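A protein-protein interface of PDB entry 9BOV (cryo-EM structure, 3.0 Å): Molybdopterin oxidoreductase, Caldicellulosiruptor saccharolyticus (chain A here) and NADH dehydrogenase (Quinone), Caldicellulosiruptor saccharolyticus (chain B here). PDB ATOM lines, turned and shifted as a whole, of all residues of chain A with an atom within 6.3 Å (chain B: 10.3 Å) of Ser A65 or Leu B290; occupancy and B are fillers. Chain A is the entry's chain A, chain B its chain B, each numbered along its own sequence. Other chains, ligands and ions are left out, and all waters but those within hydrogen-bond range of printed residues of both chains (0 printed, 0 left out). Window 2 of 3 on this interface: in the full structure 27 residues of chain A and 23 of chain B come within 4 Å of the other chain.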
ATOM      1  N   THR A  20      -7.993  -6.066  -9.024  1.00  0.00           N
ATOM      2  CA  THR A  20      -6.804  -5.264  -9.251  1.00  0.00           C
ATOM      3  C   THR A  20      -5.556  -6.128  -9.113  1.00  0.00           C
ATOM      4  O   THR A  20      -5.585  -7.223  -8.546  1.00  0.00           O
ATOM      5  CB  THR A  20      -6.742  -4.089  -8.276  1.00  0.00           C
ATOM      6  OG1 THR A  20      -6.778  -4.578  -6.931  1.00  0.00           O
ATOM      7  CG2 THR A  20      -7.914  -3.154  -8.498  1.00  0.00           C
ATOM      8  N   ILE A  21      -4.446  -5.624  -9.655  1.00  0.00           N
ATOM      9  CA  ILE A  21      -3.183  -6.346  -9.558  1.00  0.00           C
ATOM     10  C   ILE A  21      -2.755  -6.482  -8.105  1.00  0.00           C
ATOM     11  O   ILE A  21      -2.144  -7.487  -7.719  1.00  0.00           O
ATOM     12  CB  ILE A  21      -2.101  -5.651 -10.405  1.00  0.00           C
ATOM     13  CG1 ILE A  21      -2.592  -5.455 -11.837  1.00  0.00           C
ATOM     14  CG2 ILE A  21      -0.817  -6.456 -10.399  1.00  0.00           C
ATOM     15  CD1 ILE A  21      -1.618  -4.722 -12.713  1.00  0.00           C
ATOM     16  N   LEU A  22      -3.069  -5.484  -7.277  1.00  0.00           N
ATOM     17  CA  LEU A  22      -2.718  -5.552  -5.863  1.00  0.00           C
ATOM     18  C   LEU A  22      -3.408  -6.721  -5.173  1.00  0.00           C
ATOM     19  O   LEU A  22      -2.775  -7.461  -4.413  1.00  0.00           O
ATOM     20  CB  LEU A  22      -3.074  -4.236  -5.174  1.00  0.00           C
ATOM     21  CG  LEU A  22      -2.304  -3.874  -3.906  1.00  0.00           C
ATOM     22  CD1 LEU A  22      -0.884  -4.384  -3.981  1.00  0.00           C
ATOM     23  CD2 LEU A  22      -2.311  -2.375  -3.714  1.00  0.00           C
ATOM     24  N   PRO A  43      -9.678   3.915  -5.159  1.00  0.00           N
ATOM     25  CA  PRO A  43      -8.252   4.182  -5.380  1.00  0.00           C
ATOM     26  C   PRO A  43      -7.946   5.670  -5.424  1.00  0.00           C
ATOM     27  O   PRO A  43      -8.762   6.487  -5.853  1.00  0.00           O
ATOM     28  CB  PRO A  43      -7.974   3.515  -6.731  1.00  0.00           C
ATOM     29  CG  PRO A  43      -9.013   2.459  -6.843  1.00  0.00           C
ATOM     30  CD  PRO A  43     -10.237   3.038  -6.202  1.00  0.00           C
ATOM     31  N   TYR A  44      -6.744   6.014  -4.964  1.00  0.00           N
ATOM     32  CA  TYR A  44      -6.294   7.396  -4.876  1.00  0.00           C
ATOM     33  C   TYR A  44      -5.145   7.682  -5.835  1.00  0.00           C
ATOM     34  O   TYR A  44      -5.234   8.602  -6.653  1.00  0.00           O
ATOM     35  CB  TYR A  44      -5.880   7.706  -3.434  1.00  0.00           C
ATOM     36  CG  TYR A  44      -5.932   9.167  -3.064  1.00  0.00           C
ATOM     37  CD1 TYR A  44      -7.072   9.920  -3.293  1.00  0.00           C
ATOM     38  CD2 TYR A  44      -4.843   9.788  -2.475  1.00  0.00           C
ATOM     39  CE1 TYR A  44      -7.121  11.253  -2.951  1.00  0.00           C
ATOM     40  CE2 TYR A  44      -4.884  11.119  -2.132  1.00  0.00           C
ATOM     41  CZ  TYR A  44      -6.025  11.846  -2.371  1.00  0.00           C
ATOM     42  OH  TYR A  44      -6.067  13.175  -2.028  1.00  0.00           O
ATOM     43  N   GLY A  45      -4.063   6.914  -5.757  1.00  0.00           N
ATOM     44  CA  GLY A  45      -2.951   7.072  -6.672  1.00  0.00           C
ATOM     45  C   GLY A  45      -1.886   8.057  -6.252  1.00  0.00           C
ATOM     46  O   GLY A  45      -1.074   8.459  -7.091  1.00  0.00           O
ATOM     47  N   CYS A  50       3.080   1.434  -5.644  1.00  0.00           N
ATOM     48  CA  CYS A  50       2.604   0.172  -6.187  1.00  0.00           C
ATOM     49  C   CYS A  50       2.775   0.073  -7.696  1.00  0.00           C
ATOM     50  O   CYS A  50       2.065  -0.707  -8.339  1.00  0.00           O
ATOM     51  CB  CYS A  50       1.136  -0.034  -5.819  1.00  0.00           C
ATOM     52  SG  CYS A  50       0.059   1.277  -6.414  1.00  0.00           S
ATOM     53  N   ARG A  62      -0.074   1.508 -11.841  1.00  0.00           N
ATOM     54  CA  ARG A  62      -0.343   1.355 -10.419  1.00  0.00           C
ATOM     55  C   ARG A  62      -1.104   0.061 -10.167  1.00  0.00           C
ATOM     56  O   ARG A  62      -2.139  -0.193 -10.788  1.00  0.00           O
ATOM     57  CB  ARG A  62      -1.143   2.549  -9.905  1.00  0.00           C
ATOM     58  CG  ARG A  62      -0.328   3.816  -9.759  1.00  0.00           C
ATOM     59  CD  ARG A  62      -1.169   5.051 -10.017  1.00  0.00           C
ATOM     60  NE  ARG A  62      -0.495   6.256  -9.555  1.00  0.00           N
ATOM     61  CZ  ARG A  62       0.180   7.085 -10.339  1.00  0.00           C
ATOM     62  NH1 ARG A  62       0.281   6.875 -11.641  1.00  0.00           N
ATOM     63  NH2 ARG A  62       0.772   8.147  -9.805  1.00  0.00           N
ATOM     64  N   ALA A  63      -0.591  -0.759  -9.250  1.00  0.00           N
ATOM     65  CA  ALA A  63      -1.240  -2.027  -8.950  1.00  0.00           C
ATOM     66  C   ALA A  63      -2.523  -1.846  -8.152  1.00  0.00           C
ATOM     67  O   ALA A  63      -3.358  -2.754  -8.133  1.00  0.00           O
ATOM     68  CB  ALA A  63      -0.281  -2.942  -8.190  1.00  0.00           C
ATOM     69  N   CYS A  64      -2.698  -0.700  -7.496  1.00  0.00           N
ATOM     70  CA  CYS A  64      -3.892  -0.447  -6.703  1.00  0.00           C
ATOM     71  C   CYS A  64      -5.084  -0.020  -7.546  1.00  0.00           C
ATOM     72  O   CYS A  64      -6.203   0.025  -7.024  1.00  0.00           O
ATOM     73  CB  CYS A  64      -3.603   0.624  -5.648  1.00  0.00           C
ATOM     74  SG  CYS A  64      -3.434   2.303  -6.291  1.00  0.00           S
ATOM     75  N   SER A  65      -4.878   0.284  -8.819  1.00  0.00           N
ATOM     76  CA  SER A  65      -5.944   0.746  -9.698  1.00  0.00           C
ATOM     77  C   SER A  65      -6.088  -0.084 -10.961  1.00  0.00           C
ATOM     78  O   SER A  65      -7.209  -0.275 -11.439  1.00  0.00           O
ATOM     79  CB  SER A  65      -5.705   2.208 -10.083  1.00  0.00           C
ATOM     80  OG  SER A  65      -5.168   2.938  -8.996  1.00  0.00           O
ATOM     81  N   THR A  66      -4.986  -0.573 -11.522  1.00  0.00           N
ATOM     82  CA  THR A  66      -5.057  -1.358 -12.746  1.00  0.00           C
ATOM     83  C   THR A  66      -5.730  -2.697 -12.483  1.00  0.00           C
ATOM     84  O   THR A  66      -5.430  -3.379 -11.501  1.00  0.00           O
ATOM     85  CB  THR A  66      -3.658  -1.580 -13.318  1.00  0.00           C
ATOM     86  OG1 THR A  66      -2.900  -0.371 -13.207  1.00  0.00           O
ATOM     87  CG2 THR A  66      -3.736  -1.984 -14.777  1.00  0.00           C
ATOM     88  N   TYR A  67      -6.644  -3.071 -13.371  1.00  0.00           N
ATOM     89  CA  TYR A  67      -7.364  -4.332 -13.276  1.00  0.00           C
ATOM     90  C   TYR A  67      -6.688  -5.374 -14.153  1.00  0.00           C
ATOM     91  O   TYR A  67      -6.287  -5.082 -15.283  1.00  0.00           O
ATOM     92  CB  TYR A  67      -8.823  -4.162 -13.700  1.00  0.00           C
ATOM     93  CG  TYR A  67      -9.646  -3.329 -12.747  1.00  0.00           C
ATOM     94  CD1 TYR A  67     -10.146  -3.874 -11.574  1.00  0.00           C
ATOM     95  CD2 TYR A  67      -9.925  -1.999 -13.022  1.00  0.00           C
ATOM     96  CE1 TYR A  67     -10.898  -3.117 -10.700  1.00  0.00           C
ATOM     97  CE2 TYR A  67     -10.676  -1.235 -12.154  1.00  0.00           C
ATOM     98  CZ  TYR A  67     -11.159  -1.798 -10.995  1.00  0.00           C
ATOM     99  OH  TYR A  67     -11.909  -1.039 -10.126  1.00  0.00           O
ATOM    100  N   GLU B 273      -7.372  21.324 -15.657  1.00  0.00           N
ATOM    101  CA  GLU B 273      -7.379  19.914 -16.012  1.00  0.00           C
ATOM    102  C   GLU B 273      -8.801  19.375 -16.016  1.00  0.00           C
ATOM    103  O   GLU B 273      -9.637  19.788 -15.208  1.00  0.00           O
ATOM    104  CB  GLU B 273      -6.521  19.120 -15.028  1.00  0.00           C
ATOM    105  CG  GLU B 273      -6.569  17.622 -15.242  1.00  0.00           C
ATOM    106  CD  GLU B 273      -5.200  17.002 -15.341  1.00  0.00           C
ATOM    107  OE1 GLU B 273      -4.253  17.564 -14.754  1.00  0.00           O
ATOM    108  OE2 GLU B 273      -5.071  15.956 -16.008  1.00  0.00           O
ATOM    109  N   GLU B 274      -9.072  18.456 -16.947  1.00  0.00           N
ATOM    110  CA  GLU B 274     -10.389  17.840 -17.063  1.00  0.00           C
ATOM    111  C   GLU B 274     -10.924  17.365 -15.717  1.00  0.00           C
ATOM    112  O   GLU B 274     -11.998  17.786 -15.277  1.00  0.00           O
ATOM    113  CB  GLU B 274     -10.329  16.671 -18.041  1.00  0.00           C
ATOM    114  CG  GLU B 274     -10.900  16.975 -19.394  1.00  0.00           C
ATOM    115  CD  GLU B 274     -10.909  15.763 -20.288  1.00  0.00           C
ATOM    116  OE1 GLU B 274     -10.421  14.700 -19.850  1.00  0.00           O
ATOM    117  OE2 GLU B 274     -11.420  15.865 -21.423  1.00  0.00           O
ATOM    118  N   THR B 275     -10.190  16.468 -15.059  1.00  0.00           N
ATOM    119  CA  THR B 275     -10.692  15.864 -13.829  1.00  0.00           C
ATOM    120  C   THR B 275     -10.788  16.887 -12.703  1.00  0.00           C
ATOM    121  O   THR B 275     -11.755  16.882 -11.929  1.00  0.00           O
ATOM    122  CB  THR B 275      -9.803  14.690 -13.430  1.00  0.00           C
ATOM    123  OG1 THR B 275      -8.429  15.068 -13.555  1.00  0.00           O
ATOM    124  CG2 THR B 275     -10.072  13.501 -14.333  1.00  0.00           C
ATOM    125  N   ALA B 276      -9.804  17.781 -12.598  1.00  0.00           N
ATOM    126  CA  ALA B 276      -9.897  18.844 -11.607  1.00  0.00           C
ATOM    127  C   ALA B 276     -11.024  19.812 -11.935  1.00  0.00           C
ATOM    128  O   ALA B 276     -11.667  20.339 -11.022  1.00  0.00           O
ATOM    129  CB  ALA B 276      -8.570  19.588 -11.503  1.00  0.00           C
ATOM    130  N   ILE B 278     -13.818  18.904 -13.345  1.00  0.00           N
ATOM    131  CA  ILE B 278     -15.000  18.159 -12.925  1.00  0.00           C
ATOM    132  C   ILE B 278     -15.182  18.259 -11.416  1.00  0.00           C
ATOM    133  O   ILE B 278     -16.296  18.465 -10.921  1.00  0.00           O
ATOM    134  CB  ILE B 278     -14.882  16.695 -13.388  1.00  0.00           C
ATOM    135  CG1 ILE B 278     -15.222  16.580 -14.872  1.00  0.00           C
ATOM    136  CG2 ILE B 278     -15.762  15.787 -12.554  1.00  0.00           C
ATOM    137  CD1 ILE B 278     -14.447  15.503 -15.578  1.00  0.00           C
ATOM    138  N   ALA B 279     -14.089  18.119 -10.666  1.00  0.00           N
ATOM    139  CA  ALA B 279     -14.171  18.221  -9.212  1.00  0.00           C
ATOM    140  C   ALA B 279     -14.571  19.625  -8.774  1.00  0.00           C
ATOM    141  O   ALA B 279     -15.347  19.790  -7.826  1.00  0.00           O
ATOM    142  CB  ALA B 279     -12.841  17.821  -8.580  1.00  0.00           C
ATOM    143  N   MET B 287      -8.490  18.678  -7.242  1.00  0.00           N
ATOM    144  CA  MET B 287      -7.479  17.637  -7.170  1.00  0.00           C
ATOM    145  C   MET B 287      -7.725  16.646  -8.293  1.00  0.00           C
ATOM    146  O   MET B 287      -8.748  15.945  -8.270  1.00  0.00           O
ATOM    147  CB  MET B 287      -7.525  16.935  -5.816  1.00  0.00           C
ATOM    148  CG  MET B 287      -6.388  17.314  -4.888  1.00  0.00           C
ATOM    149  SD  MET B 287      -6.802  17.073  -3.155  1.00  0.00           S
ATOM    150  CE  MET B 287      -5.265  17.555  -2.374  1.00  0.00           C
ATOM    151  N   PRO B 288      -6.848  16.559  -9.292  1.00  0.00           N
ATOM    152  CA  PRO B 288      -7.088  15.634 -10.404  1.00  0.00           C
ATOM    153  C   PRO B 288      -7.198  14.195  -9.927  1.00  0.00           C
ATOM    154  O   PRO B 288      -6.453  13.748  -9.054  1.00  0.00           O
ATOM    155  CB  PRO B 288      -5.862  15.833 -11.300  1.00  0.00           C
ATOM    156  CG  PRO B 288      -5.386  17.196 -10.980  1.00  0.00           C
ATOM    157  CD  PRO B 288      -5.663  17.399  -9.522  1.00  0.00           C
ATOM    158  N   ARG B 289      -8.141  13.469 -10.516  1.00  0.00           N
ATOM    159  CA  ARG B 289      -8.350  12.065 -10.219  1.00  0.00           C
ATOM    160  C   ARG B 289      -7.685  11.219 -11.298  1.00  0.00           C
ATOM    161  O   ARG B 289      -7.093  11.733 -12.249  1.00  0.00           O
ATOM    162  CB  ARG B 289      -9.845  11.761 -10.105  1.00  0.00           C
ATOM    163  CG  ARG B 289     -10.514  12.413  -8.907  1.00  0.00           C
ATOM    164  CD  ARG B 289     -11.174  13.727  -9.290  1.00  0.00           C
ATOM    165  NE  ARG B 289     -12.404  13.521 -10.044  1.00  0.00           N
ATOM    166  CZ  ARG B 289     -13.619  13.736  -9.562  1.00  0.00           C
ATOM    167  NH1 ARG B 289     -13.805  14.176  -8.328  1.00  0.00           N
ATOM    168  NH2 ARG B 289     -14.675  13.508 -10.337  1.00  0.00           N
ATOM    169  N   LEU B 290      -7.777   9.902 -11.147  1.00  0.00           N
ATOM    170  CA  LEU B 290      -7.132   9.011 -12.099  1.00  0.00           C
ATOM    171  C   LEU B 290      -7.834   9.068 -13.448  1.00  0.00           C
ATOM    172  O   LEU B 290      -9.057   9.211 -13.527  1.00  0.00           O
ATOM    173  CB  LEU B 290      -7.110   7.582 -11.572  1.00  0.00           C
ATOM    174  CG  LEU B 290      -5.736   6.933 -11.719  1.00  0.00           C
ATOM    175  CD1 LEU B 290      -4.702   7.688 -10.903  1.00  0.00           C
ATOM    176  CD2 LEU B 290      -5.788   5.485 -11.304  1.00  0.00           C
ATOM    177  N   LYS B 291      -7.046   8.955 -14.508  1.00  0.00           N
ATOM    178  CA  LYS B 291      -7.484   9.163 -15.884  1.00  0.00           C
ATOM    179  C   LYS B 291      -8.239   7.991 -16.518  1.00  0.00           C
ATOM    180  O   LYS B 291      -9.211   8.239 -17.242  1.00  0.00           O
ATOM    181  CB  LYS B 291      -6.279   9.533 -16.751  1.00  0.00           C
ATOM    182  CG  LYS B 291      -6.599  10.521 -17.860  1.00  0.00           C
ATOM    183  CD  LYS B 291      -7.533  11.616 -17.376  1.00  0.00           C
ATOM    184  CE  LYS B 291      -8.039  12.450 -18.537  1.00  0.00           C
ATOM    185  NZ  LYS B 291      -8.483  13.802 -18.106  1.00  0.00           N
ATOM    186  N   PRO B 292      -7.838   6.730 -16.317  1.00  0.00           N
ATOM    187  CA  PRO B 292      -8.448   5.622 -17.082  1.00  0.00           C
ATOM    188  C   PRO B 292      -9.964   5.597 -16.982  1.00  0.00           C
ATOM    189  O   PRO B 292     -10.634   5.273 -17.974  1.00  0.00           O
ATOM    190  CB  PRO B 292      -7.821   4.376 -16.449  1.00  0.00           C
ATOM    191  CG  PRO B 292      -6.485   4.828 -16.059  1.00  0.00           C
ATOM    192  CD  PRO B 292      -6.635   6.260 -15.604  1.00  0.00           C
ATOM    193  N   PRO B 293     -10.568   5.926 -15.821  1.00  0.00           N
ATOM    194  CA  PRO B 293     -12.000   6.252 -15.860  1.00  0.00           C
ATOM    195  C   PRO B 293     -12.194   7.605 -16.519  1.00  0.00           C
ATOM    196  O   PRO B 293     -11.913   8.645 -15.917  1.00  0.00           O
ATOM    197  CB  PRO B 293     -12.410   6.266 -14.382  1.00  0.00           C
ATOM    198  CG  PRO B 293     -11.348   5.507 -13.680  1.00  0.00           C
ATOM    199  CD  PRO B 293     -10.094   5.797 -14.433  1.00  0.00           C
ATOM    200  N   PHE B 294     -12.667   7.600 -17.732  1.00  0.00           N
ATOM    201  CA  PHE B 294     -12.560   8.830 -18.499  1.00  0.00           C
ATOM    202  C   PHE B 294     -13.833   9.661 -18.390  1.00  0.00           C
ATOM    203  O   PHE B 294     -14.918   9.120 -18.154  1.00  0.00           O
ATOM    204  CB  PHE B 294     -12.280   8.510 -19.961  1.00  0.00           C
ATOM    205  CG  PHE B 294     -10.820   8.390 -20.284  1.00  0.00           C
ATOM    206  CD1 PHE B 294      -9.984   9.488 -20.195  1.00  0.00           C
ATOM    207  CD2 PHE B 294     -10.284   7.179 -20.675  1.00  0.00           C
ATOM    208  CE1 PHE B 294      -8.641   9.379 -20.492  1.00  0.00           C
ATOM    209  CE2 PHE B 294      -8.940   7.064 -20.973  1.00  0.00           C
ATOM    210  CZ  PHE B 294      -8.119   8.166 -20.882  1.00  0.00           C
ATOM    211  N   PRO B 295     -13.715  10.983 -18.546  1.00  0.00           N
ATOM    212  CA  PRO B 295     -14.916  11.829 -18.522  1.00  0.00           C
ATOM    213  C   PRO B 295     -15.931  11.462 -19.586  1.00  0.00           C
ATOM    214  O   PRO B 295     -17.136  11.630 -19.363  1.00  0.00           O
ATOM    215  CB  PRO B 295     -14.347  13.237 -18.738  1.00  0.00           C
ATOM    216  CG  PRO B 295     -12.967  13.152 -18.215  1.00  0.00           C
ATOM    217  CD  PRO B 295     -12.485  11.787 -18.594  1.00  0.00           C
ATOM    218  N   ALA B 296     -15.482  10.962 -20.739  1.00  0.00           N
ATOM    219  CA  ALA B 296     -16.412  10.505 -21.761  1.00  0.00           C
ATOM    220  C   ALA B 296     -17.227   9.307 -21.298  1.00  0.00           C
ATOM    221  O   ALA B 296     -18.308   9.060 -21.842  1.00  0.00           O
ATOM    222  CB  ALA B 296     -15.659  10.161 -23.044  1.00  0.00           C
ATOM    223  N   GLN B 297     -16.734   8.554 -20.316  1.00  0.00           N
ATOM    224  CA  GLN B 297     -17.469   7.426 -19.763  1.00  0.00           C
ATOM    225  C   GLN B 297     -17.975   7.665 -18.351  1.00  0.00           C
ATOM    226  O   GLN B 297     -18.997   7.090 -17.972  1.00  0.00           O
ATOM    227  CB  GLN B 297     -16.596   6.167 -19.765  1.00  0.00           C
ATOM    228  CG  GLN B 297     -15.756   6.001 -21.017  1.00  0.00           C
ATOM    229  CD  GLN B 297     -16.475   5.237 -22.109  1.00  0.00           C
ATOM    230  OE1 GLN B 297     -17.701   5.143 -22.115  1.00  0.00           O
ATOM    231  NE2 GLN B 297     -15.711   4.688 -23.045  1.00  0.00           N
ATOM    232  N   SER B 298     -17.283   8.489 -17.562  1.00  0.00           N
ATOM    233  CA  SER B 298     -17.760   8.847 -16.226  1.00  0.00           C
ATOM    234  C   SER B 298     -17.133  10.192 -15.861  1.00  0.00           C
ATOM    235  O   SER B 298     -15.967  10.242 -15.466  1.00  0.00           O
ATOM    236  CB  SER B 298     -17.408   7.774 -15.212  1.00  0.00           C
ATOM    237  OG  SER B 298     -17.704   8.201 -13.894  1.00  0.00           O
ATOM    238  N   GLY B 299     -17.913  11.261 -15.983  1.00  0.00           N
ATOM    239  CA  GLY B 299     -17.406  12.587 -15.696  1.00  0.00           C
ATOM    240  C   GLY B 299     -18.109  13.275 -14.546  1.00  0.00           C
ATOM    241  O   GLY B 299     -17.934  12.897 -13.385  1.00  0.00           O
ATOM    242  N   LYS B 444      -1.146  16.263  -4.379  1.00  0.00           N
ATOM    243  CA  LYS B 444      -1.644  14.922  -4.094  1.00  0.00           C
ATOM    244  C   LYS B 444      -0.520  13.891  -4.122  1.00  0.00           C
ATOM    245  O   LYS B 444      -0.277  13.199  -3.129  1.00  0.00           O
ATOM    246  CB  LYS B 444      -2.745  14.547  -5.087  1.00  0.00           C
ATOM    247  CG  LYS B 444      -3.080  13.067  -5.096  1.00  0.00           C
ATOM    248  CD  LYS B 444      -3.835  12.678  -6.350  1.00  0.00           C
ATOM    249  CE  LYS B 444      -5.328  12.836  -6.159  1.00  0.00           C
ATOM    250  NZ  LYS B 444      -6.094  12.008  -7.127  1.00  0.00           N
ATOM    251  N   CYS B 445       0.182  13.779  -5.247  1.00  0.00           N
ATOM    252  CA  CYS B 445       1.194  12.745  -5.410  1.00  0.00           C
ATOM    253  C   CYS B 445       2.576  13.273  -5.050  1.00  0.00           C
ATOM    254  O   CYS B 445       2.878  14.455  -5.223  1.00  0.00           O
ATOM    255  CB  CYS B 445       1.200  12.202  -6.839  1.00  0.00           C
ATOM    256  SG  CYS B 445       1.353  13.442  -8.123  1.00  0.00           S
ATOM    257  N   GLY B 485       6.569   9.732 -13.199  1.00  0.00           N
ATOM    258  CA  GLY B 485       5.951   9.219 -11.993  1.00  0.00           C
ATOM    259  C   GLY B 485       4.760  10.019 -11.511  1.00  0.00           C
ATOM    260  O   GLY B 485       3.952   9.517 -10.726  1.00  0.00           O
ATOM    261  N   SER B 486       4.635  11.259 -11.972  1.00  0.00           N
ATOM    262  CA  SER B 486       3.548  12.109 -11.520  1.00  0.00           C
ATOM    263  C   SER B 486       2.211  11.592 -12.038  1.00  0.00           C
ATOM    264  O   SER B 486       2.133  10.885 -13.046  1.00  0.00           O
ATOM    265  CB  SER B 486       3.767  13.550 -11.974  1.00  0.00           C
ATOM    266  OG  SER B 486       5.023  14.033 -11.540  1.00  0.00           O
ATOM    267  N   LEU B 487       1.144  11.959 -11.330  1.00  0.00           N
ATOM    268  CA  LEU B 487      -0.178  11.434 -11.651  1.00  0.00           C
ATOM    269  C   LEU B 487      -0.812  12.190 -12.811  1.00  0.00           C
ATOM    270  O   LEU B 487      -1.164  11.590 -13.831  1.00  0.00           O
ATOM    271  CB  LEU B 487      -1.076  11.495 -10.413  1.00  0.00           C
ATOM    272  CG  LEU B 487      -2.390  10.712 -10.412  1.00  0.00           C
ATOM    273  CD1 LEU B 487      -2.779  10.356  -8.993  1.00  0.00           C
ATOM    274  CD2 LEU B 487      -3.512  11.493 -11.072  1.00  0.00           C
ATOM    275  N   CYS B 488      -0.969  13.500 -12.673  1.00  0.00           N
ATOM    276  CA  CYS B 488      -1.686  14.297 -13.652  1.00  0.00           C
ATOM    277  C   CYS B 488      -0.709  14.953 -14.620  1.00  0.00           C
ATOM    278  O   CYS B 488       0.509  14.775 -14.538  1.00  0.00           O
ATOM    279  CB  CYS B 488      -2.553  15.341 -12.953  1.00  0.00           C
ATOM    280  SG  CYS B 488      -1.760  16.934 -12.753  1.00  0.00           S
ATOM    281  N   GLY B 489      -1.258  15.728 -15.557  1.00  0.00           N
ATOM    282  CA  GLY B 489      -0.436  16.366 -16.567  1.00  0.00           C
ATOM    283  C   GLY B 489       0.329  17.579 -16.087  1.00  0.00           C
ATOM    284  O   GLY B 489       1.240  18.034 -16.783  1.00  0.00           O
ATOM    285  N   GLN B 492       3.576  15.675 -15.012  1.00  0.00           N
ATOM    286  CA  GLN B 492       4.255  15.041 -16.135  1.00  0.00           C
ATOM    287  C   GLN B 492       4.836  16.071 -17.094  1.00  0.00           C
ATOM    288  O   GLN B 492       5.783  15.768 -17.826  1.00  0.00           O
ATOM    289  CB  GLN B 492       3.293  14.115 -16.877  1.00  0.00           C
ATOM    290  CG  GLN B 492       2.800  12.944 -16.054  1.00  0.00           C
ATOM    291  CD  GLN B 492       1.715  12.160 -16.759  1.00  0.00           C
ATOM    292  OE1 GLN B 492       1.242  12.557 -17.821  1.00  0.00           O
ATOM    293  NE2 GLN B 492       1.313  11.041 -16.170  1.00  0.00           N
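O of Gly A45 lies within hydrogen-bond range of NH2 of Arg A62 (3.3 Å).
The backbone carbonyl oxygen (O) of Arg A62 is in hydrogen-bond range of the side-chain hydroxyl (OG1) of Thr A66 (2.5 Å).
SG of Cys A64 sits close to OG of Ser A65 (3.3 Å).
The side-chain amino group (NZ) of Lys B444 sits at hydrogen-bond distance from the backbone carbonyl oxygen (O) of Pro B288, 2.6 Å away.
The backbone NH (N) of Leu B487 sits close to the side-chain sulfur (SG) of Cys B445, 3.5 Å away.
O of Leu B487 lies within hydrogen-bond range of NE2 of Gln B492 (3.5 Å).
Hydrophobic or aromatic side chains of chain B within 4 Å of the printed part of chain A: Leu B290 and Leu B487.
Hydrophobic or aromatic side chains of chain A that line the printed part of chain B: Tyr A44.
Among the printed residues, 6 pairs touch across the chains.
Ser A65 touches just one residue of chain B: Leu B290 (3.5 Å).
Printed residues of chain A within 4 Å of Leu B290: Ser A65 (3.5 Å).
No residue of chain B comes within 4 Å of Pro A43.
Gly A45 touches one residue of chain B.
Of chain B, only Gly B485 and Leu B487 come within 4 Å of Arg A62.
No residue of chain B comes within 4 Å of Cys A64.
Thr A66 touches none of the printed residues of chain B.
Tyr A67 touches none of the printed residues of chain B.
Of the printed residues of chain A, Lys B444 touches Tyr A44 (3.5 Å).
Printed residues of chain A within 4 Å of Leu B487: Tyr A44 (3.8 Å), Gly A45 (3.2 Å) and Arg A62 (3.9 Å).
Of the printed residues of chain A, Gly B485 touches Arg A62.
Printed residues of chain B within 4 Å of Tyr A44: Lys B444 and Leu B487.
The nearest residue of chain A that does not touch Leu B290 is Tyr A44 (4.4 Å).
O of Tyr A44 touches NZ of Lys B444 (3.5 Å).
Tyr A44 touches Leu B487.
Leu B487 touches Gly A45.
Gly B485 touches Arg A62 (O to NH2, 3.6 Å).
Leu B487 touches Arg A62.
Leu B290 touches Ser A65 (CD2 to OG, 3.5 Å).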
